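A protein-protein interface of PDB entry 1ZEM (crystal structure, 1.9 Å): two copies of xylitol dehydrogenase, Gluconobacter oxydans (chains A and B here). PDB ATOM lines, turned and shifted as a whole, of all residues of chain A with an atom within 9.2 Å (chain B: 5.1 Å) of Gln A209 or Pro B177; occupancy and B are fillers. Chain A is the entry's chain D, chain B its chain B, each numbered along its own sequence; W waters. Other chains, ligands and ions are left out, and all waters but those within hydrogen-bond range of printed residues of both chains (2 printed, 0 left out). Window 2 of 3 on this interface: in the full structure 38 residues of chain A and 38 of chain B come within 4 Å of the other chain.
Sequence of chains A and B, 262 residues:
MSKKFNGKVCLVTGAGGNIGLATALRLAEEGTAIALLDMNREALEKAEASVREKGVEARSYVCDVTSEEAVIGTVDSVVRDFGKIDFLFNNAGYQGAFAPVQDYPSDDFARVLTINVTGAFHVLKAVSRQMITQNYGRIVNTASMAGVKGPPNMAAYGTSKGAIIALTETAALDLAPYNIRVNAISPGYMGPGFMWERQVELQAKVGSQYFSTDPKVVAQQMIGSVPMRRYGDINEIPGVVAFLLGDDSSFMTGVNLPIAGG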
ATOM      1  N   PRO A 100     -10.364  24.910  22.791  1.00  0.00           N
ATOM      2  CA  PRO A 100      -9.053  24.316  22.524  1.00  0.00           C
ATOM      3  C   PRO A 100      -9.058  23.946  21.071  1.00  0.00           C
ATOM      4  O   PRO A 100     -10.139  23.691  20.501  1.00  0.00           O
ATOM      5  CB  PRO A 100      -8.995  23.085  23.451  1.00  0.00           C
ATOM      6  CG  PRO A 100     -10.466  22.719  23.657  1.00  0.00           C
ATOM      7  CD  PRO A 100     -11.136  24.112  23.768  1.00  0.00           C
ATOM      8  N   GLN A 102      -8.581  21.262  19.172  1.00  0.00           N
ATOM      9  CA  GLN A 102      -9.310  20.069  18.757  1.00  0.00           C
ATOM     10  C   GLN A 102     -10.810  20.239  18.625  1.00  0.00           C
ATOM     11  O   GLN A 102     -11.466  19.397  17.998  1.00  0.00           O
ATOM     12  CB  GLN A 102      -9.039  18.896  19.735  1.00  0.00           C
ATOM     13  CG  GLN A 102      -9.671  19.051  21.152  1.00  0.00           C
ATOM     14  CD  GLN A 102      -8.753  19.741  22.176  1.00  0.00           C
ATOM     15  OE1 GLN A 102      -7.906  20.588  21.824  1.00  0.00           O
ATOM     16  NE2 GLN A 102      -8.954  19.413  23.458  1.00  0.00           N
ATOM     17  N   PRO A 152      -3.759  30.011  25.112  1.00  0.00           N
ATOM     18  CA  PRO A 152      -4.565  28.803  25.113  1.00  0.00           C
ATOM     19  C   PRO A 152      -6.026  29.161  24.662  1.00  0.00           C
ATOM     20  O   PRO A 152      -6.550  30.245  24.974  1.00  0.00           O
ATOM     21  CB  PRO A 152      -4.475  28.358  26.583  1.00  0.00           C
ATOM     22  CG  PRO A 152      -4.372  29.596  27.325  1.00  0.00           C
ATOM     23  CD  PRO A 152      -3.430  30.430  26.487  1.00  0.00           C
ATOM     24  N   ASN A 153      -6.634  28.244  23.931  1.00  0.00           N
ATOM     25  CA  ASN A 153      -7.972  28.332  23.427  1.00  0.00           C
ATOM     26  C   ASN A 153      -8.235  29.481  22.427  1.00  0.00           C
ATOM     27  O   ASN A 153      -9.412  29.804  22.131  1.00  0.00           O
ATOM     28  CB  ASN A 153      -8.952  28.393  24.618  1.00  0.00           C
ATOM     29  CG  ASN A 153      -8.645  27.321  25.665  1.00  0.00           C
ATOM     30  OD1 ASN A 153      -8.689  26.139  25.350  1.00  0.00           O
ATOM     31  ND2 ASN A 153      -8.287  27.734  26.898  1.00  0.00           N
ATOM     32  N   GLN A 203     -13.055  32.218  28.549  1.00  0.00           N
ATOM     33  CA  GLN A 203     -11.928  31.343  28.921  1.00  0.00           C
ATOM     34  C   GLN A 203     -12.456  30.499  30.071  1.00  0.00           C
ATOM     35  O   GLN A 203     -12.182  29.280  30.161  1.00  0.00           O
ATOM     36  CB  GLN A 203     -10.717  32.157  29.441  1.00  0.00           C
ATOM     37  CG  GLN A 203      -9.846  32.741  28.377  1.00  0.00           C
ATOM     38  CD  GLN A 203      -8.972  31.685  27.670  1.00  0.00           C
ATOM     39  OE1 GLN A 203      -9.136  30.477  27.861  1.00  0.00           O
ATOM     40  NE2 GLN A 203      -8.060  32.154  26.837  1.00  0.00           N
ATOM     41  N   ALA A 204     -13.240  31.127  30.951  1.00  0.00           N
ATOM     42  CA  ALA A 204     -13.745  30.365  32.078  1.00  0.00           C
ATOM     43  C   ALA A 204     -14.586  29.183  31.614  1.00  0.00           C
ATOM     44  O   ALA A 204     -14.406  28.077  32.080  1.00  0.00           O
ATOM     45  CB  ALA A 204     -14.532  31.256  33.041  1.00  0.00           C
ATOM     46  N   VAL A 206     -14.377  27.467  28.972  1.00  0.00           N
ATOM     47  CA  VAL A 206     -13.652  26.339  28.399  1.00  0.00           C
ATOM     48  C   VAL A 206     -13.299  25.231  29.397  1.00  0.00           C
ATOM     49  O   VAL A 206     -13.506  24.063  29.114  1.00  0.00           O
ATOM     50  CB  VAL A 206     -12.300  26.777  27.707  1.00  0.00           C
ATOM     51  CG1 VAL A 206     -11.499  25.546  27.225  1.00  0.00           C
ATOM     52  CG2 VAL A 206     -12.598  27.690  26.569  1.00  0.00           C
ATOM     53  N   GLY A 207     -12.777  25.599  30.567  1.00  0.00           N
ATOM     54  CA  GLY A 207     -12.386  24.587  31.528  1.00  0.00           C
ATOM     55  C   GLY A 207     -11.050  23.903  31.234  1.00  0.00           C
ATOM     56  O   GLY A 207     -10.822  22.748  31.628  1.00  0.00           O
ATOM     57  N   SER A 208     -10.158  24.594  30.532  1.00  0.00           N
ATOM     58  CA  SER A 208      -8.837  24.042  30.242  1.00  0.00           C
ATOM     59  C   SER A 208      -8.048  24.190  31.509  1.00  0.00           C
ATOM     60  O   SER A 208      -8.510  24.833  32.438  1.00  0.00           O
ATOM     61  CB  SER A 208      -8.120  24.846  29.170  1.00  0.00           C
ATOM     62  OG  SER A 208      -7.878  26.172  29.690  1.00  0.00           O
ATOM     63  N   GLN A 209      -6.837  23.613  31.534  1.00  0.00           N
ATOM     64  CA  GLN A 209      -5.960  23.669  32.710  1.00  0.00           C
ATOM     65  C   GLN A 209      -5.383  25.031  32.950  1.00  0.00           C
ATOM     66  O   GLN A 209      -4.744  25.267  33.988  1.00  0.00           O
ATOM     67  CB  GLN A 209      -4.762  22.705  32.578  1.00  0.00           C
ATOM     68  CG  GLN A 209      -3.773  23.087  31.448  1.00  0.00           C
ATOM     69  CD  GLN A 209      -2.535  22.227  31.399  1.00  0.00           C
ATOM     70  OE1 GLN A 209      -1.518  22.598  30.735  1.00  0.00           O
ATOM     71  NE2 GLN A 209      -2.576  21.071  32.073  1.00  0.00           N
ATOM     72  N   TYR A 210      -5.578  25.933  31.988  1.00  0.00           N
ATOM     73  CA  TYR A 210      -5.011  27.265  32.102  1.00  0.00           C
ATOM     74  C   TYR A 210      -5.745  28.309  32.934  1.00  0.00           C
ATOM     75  O   TYR A 210      -5.129  29.294  33.349  1.00  0.00           O
ATOM     76  CB  TYR A 210      -4.770  27.804  30.692  1.00  0.00           C
ATOM     77  CG  TYR A 210      -3.768  26.939  29.974  1.00  0.00           C
ATOM     78  CD1 TYR A 210      -2.414  26.996  30.304  1.00  0.00           C
ATOM     79  CD2 TYR A 210      -4.179  26.010  29.048  1.00  0.00           C
ATOM     80  CE1 TYR A 210      -1.490  26.131  29.728  1.00  0.00           C
ATOM     81  CE2 TYR A 210      -3.312  25.167  28.476  1.00  0.00           C
ATOM     82  CZ  TYR A 210      -1.963  25.214  28.808  1.00  0.00           C
ATOM     83  OH  TYR A 210      -1.117  24.302  28.238  1.00  0.00           O
ATOM     84  N   PHE A 211      -7.036  28.124  33.158  1.00  0.00           N
ATOM     85  CA  PHE A 211      -7.838  29.072  33.936  1.00  0.00           C
ATOM     86  C   PHE A 211      -8.965  28.364  34.678  1.00  0.00           C
ATOM     87  O   PHE A 211      -9.424  27.298  34.243  1.00  0.00           O
ATOM     88  CB  PHE A 211      -8.498  30.114  33.029  1.00  0.00           C
ATOM     89  CG  PHE A 211      -7.528  31.029  32.313  1.00  0.00           C
ATOM     90  CD1 PHE A 211      -7.235  30.845  30.963  1.00  0.00           C
ATOM     91  CD2 PHE A 211      -6.899  32.051  33.012  1.00  0.00           C
ATOM     92  CE1 PHE A 211      -6.306  31.685  30.309  1.00  0.00           C
ATOM     93  CE2 PHE A 211      -5.992  32.879  32.400  1.00  0.00           C
ATOM     94  CZ  PHE A 211      -5.687  32.697  31.025  1.00  0.00           C
ATOM     95  N   SER A 212      -9.442  28.965  35.773  1.00  0.00           N
ATOM     96  CA  SER A 212     -10.556  28.372  36.510  1.00  0.00           C
ATOM     97  C   SER A 212     -11.846  28.442  35.665  1.00  0.00           C
ATOM     98  O   SER A 212     -11.857  29.137  34.649  1.00  0.00           O
ATOM     99  CB  SER A 212     -10.782  29.154  37.799  1.00  0.00           C
ATOM    100  OG  SER A 212     -11.929  28.654  38.467  1.00  0.00           O
ATOM    101  N   THR A 213     -12.908  27.723  36.055  1.00  0.00           N
ATOM    102  CA  THR A 213     -14.186  27.827  35.341  1.00  0.00           C
ATOM    103  C   THR A 213     -14.984  28.929  36.083  1.00  0.00           C
ATOM    104  O   THR A 213     -16.069  29.303  35.671  1.00  0.00           O
ATOM    105  CB  THR A 213     -15.041  26.469  35.288  1.00  0.00           C
ATOM    106  OG1 THR A 213     -15.346  26.016  36.622  1.00  0.00           O
ATOM    107  CG2 THR A 213     -14.227  25.307  34.534  1.00  0.00           C
ATOM    108  N   GLN A 221      -6.569  35.534  37.838  1.00  0.00           N
ATOM    109  CA  GLN A 221      -5.430  34.846  37.268  1.00  0.00           C
ATOM    110  C   GLN A 221      -4.853  35.685  36.155  1.00  0.00           C
ATOM    111  O   GLN A 221      -3.637  35.794  36.026  1.00  0.00           O
ATOM    112  CB  GLN A 221      -5.863  33.484  36.726  1.00  0.00           C
ATOM    113  CG  GLN A 221      -6.486  32.627  37.818  1.00  0.00           C
ATOM    114  CD  GLN A 221      -7.052  31.311  37.308  1.00  0.00           C
ATOM    115  OE1 GLN A 221      -7.901  31.283  36.430  1.00  0.00           O
ATOM    116  NE2 GLN A 221      -6.579  30.216  37.866  1.00  0.00           N
ATOM    117  N   ASN B 135      -3.822   9.472  23.678  1.00  0.00           N
ATOM    118  CA  ASN B 135      -2.960  10.094  24.694  1.00  0.00           C
ATOM    119  C   ASN B 135      -1.508  10.006  24.194  1.00  0.00           C
ATOM    120  O   ASN B 135      -0.565   9.648  24.928  1.00  0.00           O
ATOM    121  CB  ASN B 135      -3.091   9.483  26.101  1.00  0.00           C
ATOM    122  CG  ASN B 135      -2.736  10.484  27.190  1.00  0.00           C
ATOM    123  OD1 ASN B 135      -3.467  11.472  27.404  1.00  0.00           O
ATOM    124  ND2 ASN B 135      -1.618  10.266  27.854  1.00  0.00           N
ATOM    125  N   LEU B 173      -0.001  24.531  23.726  1.00  0.00           N
ATOM    126  CA  LEU B 173      -0.650  24.742  24.992  1.00  0.00           C
ATOM    127  C   LEU B 173      -1.898  23.874  25.144  1.00  0.00           C
ATOM    128  O   LEU B 173      -2.090  23.192  26.191  1.00  0.00           O
ATOM    129  CB  LEU B 173      -1.070  26.220  25.132  1.00  0.00           C
ATOM    130  CG  LEU B 173       0.067  27.226  25.308  1.00  0.00           C
ATOM    131  CD1 LEU B 173      -0.546  28.596  25.620  1.00  0.00           C
ATOM    132  CD2 LEU B 173       0.962  26.846  26.398  1.00  0.00           C
ATOM    133  N   ASP B 174      -2.729  23.891  24.103  1.00  0.00           N
ATOM    134  CA  ASP B 174      -4.014  23.159  24.137  1.00  0.00           C
ATOM    135  C   ASP B 174      -3.868  21.648  24.275  1.00  0.00           C
ATOM    136  O   ASP B 174      -4.619  20.986  25.016  1.00  0.00           O
ATOM    137  CB  ASP B 174      -4.825  23.428  22.873  1.00  0.00           C
ATOM    138  CG  ASP B 174      -5.351  24.862  22.789  1.00  0.00           C
ATOM    139  OD1 ASP B 174      -5.871  25.199  21.710  1.00  0.00           O
ATOM    140  OD2 ASP B 174      -5.251  25.627  23.782  1.00  0.00           O
ATOM    141  N   LEU B 175      -2.868  21.123  23.585  1.00  0.00           N
ATOM    142  CA  LEU B 175      -2.650  19.690  23.544  1.00  0.00           C
ATOM    143  C   LEU B 175      -1.655  19.055  24.541  1.00  0.00           C
ATOM    144  O   LEU B 175      -1.637  17.810  24.677  1.00  0.00           O
ATOM    145  CB  LEU B 175      -2.273  19.338  22.109  1.00  0.00           C
ATOM    146  CG  LEU B 175      -3.338  19.794  21.079  1.00  0.00           C
ATOM    147  CD1 LEU B 175      -2.877  19.439  19.654  1.00  0.00           C
ATOM    148  CD2 LEU B 175      -4.720  19.095  21.382  1.00  0.00           C
ATOM    149  N   ALA B 176      -0.831  19.871  25.214  1.00  0.00           N
ATOM    150  CA  ALA B 176       0.130  19.359  26.221  1.00  0.00           C
ATOM    151  C   ALA B 176      -0.477  18.383  27.215  1.00  0.00           C
ATOM    152  O   ALA B 176       0.173  17.395  27.594  1.00  0.00           O
ATOM    153  CB  ALA B 176       0.807  20.548  27.058  1.00  0.00           C
ATOM    154  N   PRO B 177      -1.713  18.634  27.685  1.00  0.00           N
ATOM    155  CA  PRO B 177      -2.269  17.671  28.677  1.00  0.00           C
ATOM    156  C   PRO B 177      -2.503  16.241  28.240  1.00  0.00           C
ATOM    157  O   PRO B 177      -2.716  15.357  29.086  1.00  0.00           O
ATOM    158  CB  PRO B 177      -3.591  18.305  29.112  1.00  0.00           C
ATOM    159  CG  PRO B 177      -3.329  19.846  28.857  1.00  0.00           C
ATOM    160  CD  PRO B 177      -2.603  19.798  27.504  1.00  0.00           C
ATOM    161  N   TYR B 178      -2.451  15.997  26.945  1.00  0.00           N
ATOM    162  CA  TYR B 178      -2.725  14.675  26.396  1.00  0.00           C
ATOM    163  C   TYR B 178      -1.501  13.989  25.811  1.00  0.00           C
ATOM    164  O   TYR B 178      -1.621  13.139  24.930  1.00  0.00           O
ATOM    165  CB  TYR B 178      -3.765  14.819  25.322  1.00  0.00           C
ATOM    166  CG  TYR B 178      -4.919  15.682  25.724  1.00  0.00           C
ATOM    167  CD1 TYR B 178      -5.068  17.000  25.209  1.00  0.00           C
ATOM    168  CD2 TYR B 178      -5.839  15.232  26.657  1.00  0.00           C
ATOM    169  CE1 TYR B 178      -6.104  17.810  25.640  1.00  0.00           C
ATOM    170  CE2 TYR B 178      -6.856  16.032  27.095  1.00  0.00           C
ATOM    171  CZ  TYR B 178      -6.990  17.320  26.596  1.00  0.00           C
ATOM    172  OH  TYR B 178      -7.988  18.120  27.117  1.00  0.00           O
ATOM    173  N   ASN B 179      -0.321  14.371  26.295  1.00  0.00           N
ATOM    174  CA  ASN B 179       0.913  13.816  25.816  1.00  0.00           C
ATOM    175  C   ASN B 179       1.124  14.046  24.317  1.00  0.00           C
ATOM    176  O   ASN B 179       1.537  13.160  23.574  1.00  0.00           O
ATOM    177  CB  ASN B 179       1.001  12.306  26.159  1.00  0.00           C
ATOM    178  CG  ASN B 179       2.368  11.720  25.819  1.00  0.00           C
ATOM    179  OD1 ASN B 179       3.394  12.427  25.790  1.00  0.00           O
ATOM    180  ND2 ASN B 179       2.396  10.423  25.562  1.00  0.00           N
HETATM  181  O   HOH W   1      -6.359  24.873  26.235  1.00  0.00           O
HETATM  182  O   HOH W   2      -8.538  20.656  26.176  1.00  0.00           O
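The backbone carbonyl oxygen of Leu B173 lies within hydrogen-bond range of the side-chain hydroxyl of Tyr A210 (2.5 Å). The side-chain carboxylate (OD2) of Asp B174 lies within hydrogen-bond range of the backbone NH (N) of Asn A153 (3.0 Å).
Hydrophobic or aromatic side chains of chain B within 4 Å of the printed part of chain A: Leu B173, Leu B175, Pro B177 and Tyr B178. Hydrophobic or aromatic side chains of chain A within 4 Å of the printed part of chain B: Pro A152 and Tyr A210. Among the printed residues, 8 pairs touch across the chains. Among the printed residues, no Asp or Glu carboxylate lies within 4 Å of a Lys or Arg side-chain nitrogen of the other chain.
O of Pro A152 sits at hydrogen-bond distance from NE2 of Gln A203 (3.1 Å). ND2 of Asn A153 lies within hydrogen-bond range of OE1 of Gln A203. The side-chain amide nitrogen (ND2) of Asn A153 is in hydrogen-bond range of the side-chain hydroxyl (OG) of Ser A208. OG of Ser A208 sits close to N of Tyr A210, 3.3 Å away. The side-chain amide oxygen (OE1) of Gln A209 lies within hydrogen-bond range of the side-chain hydroxyl (OH) of Tyr A210 (3.0 Å).
Pro A100 touches Asp B174 (CA to OD1, 3.4 Å). CD2 of Leu B175 touches OE1 of Gln A102, 3.5 Å away. Gln A102 touches Tyr B178. Pro A152 touches Leu B173 (CD to CD1, 3.5 Å). Asp B174 touches Pro A152 (OD2 to CA, 3.5 Å). Pro B177 touches Gln A209.
Water W2 lies within hydrogen-bond range of OH of Tyr B178 (2.8 Å) and NE2 of Gln A102 (3.0 Å). Water W1 bridges OD2 of Asp B174 (2.8 Å) and OD1 of Asn A153 (2.8 Å).
No position is printed for both chains. Of the 8 pairs that touch across the chains among the printed residues, none has its exchanged pair printed and touching as well.
Of the printed residues of chain B, Gln A102 touches Leu B175 and Tyr B178. Printed residues of chain B within 4 Å of Pro A152: Leu B173 (3.5 Å) and Asp B174 (3.5 Å). Of the printed residues of chain B, Asn A153 touches Asp B174. Val A206 touches none of the printed residues of chain B. Of chain B, only Pro B177 comes within 4 Å of Gln A209. Printed residues of chain B within 4 Å of Tyr A210: Leu B173. Printed residues of chain A within 4 Å of Asp B174: Pro A100, Pro A152 and Asn A153. No residue of chain A comes within 4 Å of Ala B176. Pro B177 touches one residue of chain A. Of chain A, only Gln A102 (3.9 Å) comes within 4 Å of Tyr B178. The nearest printed residue of chain A that does not touch Leu B175 is Tyr A210 (5.9 Å).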
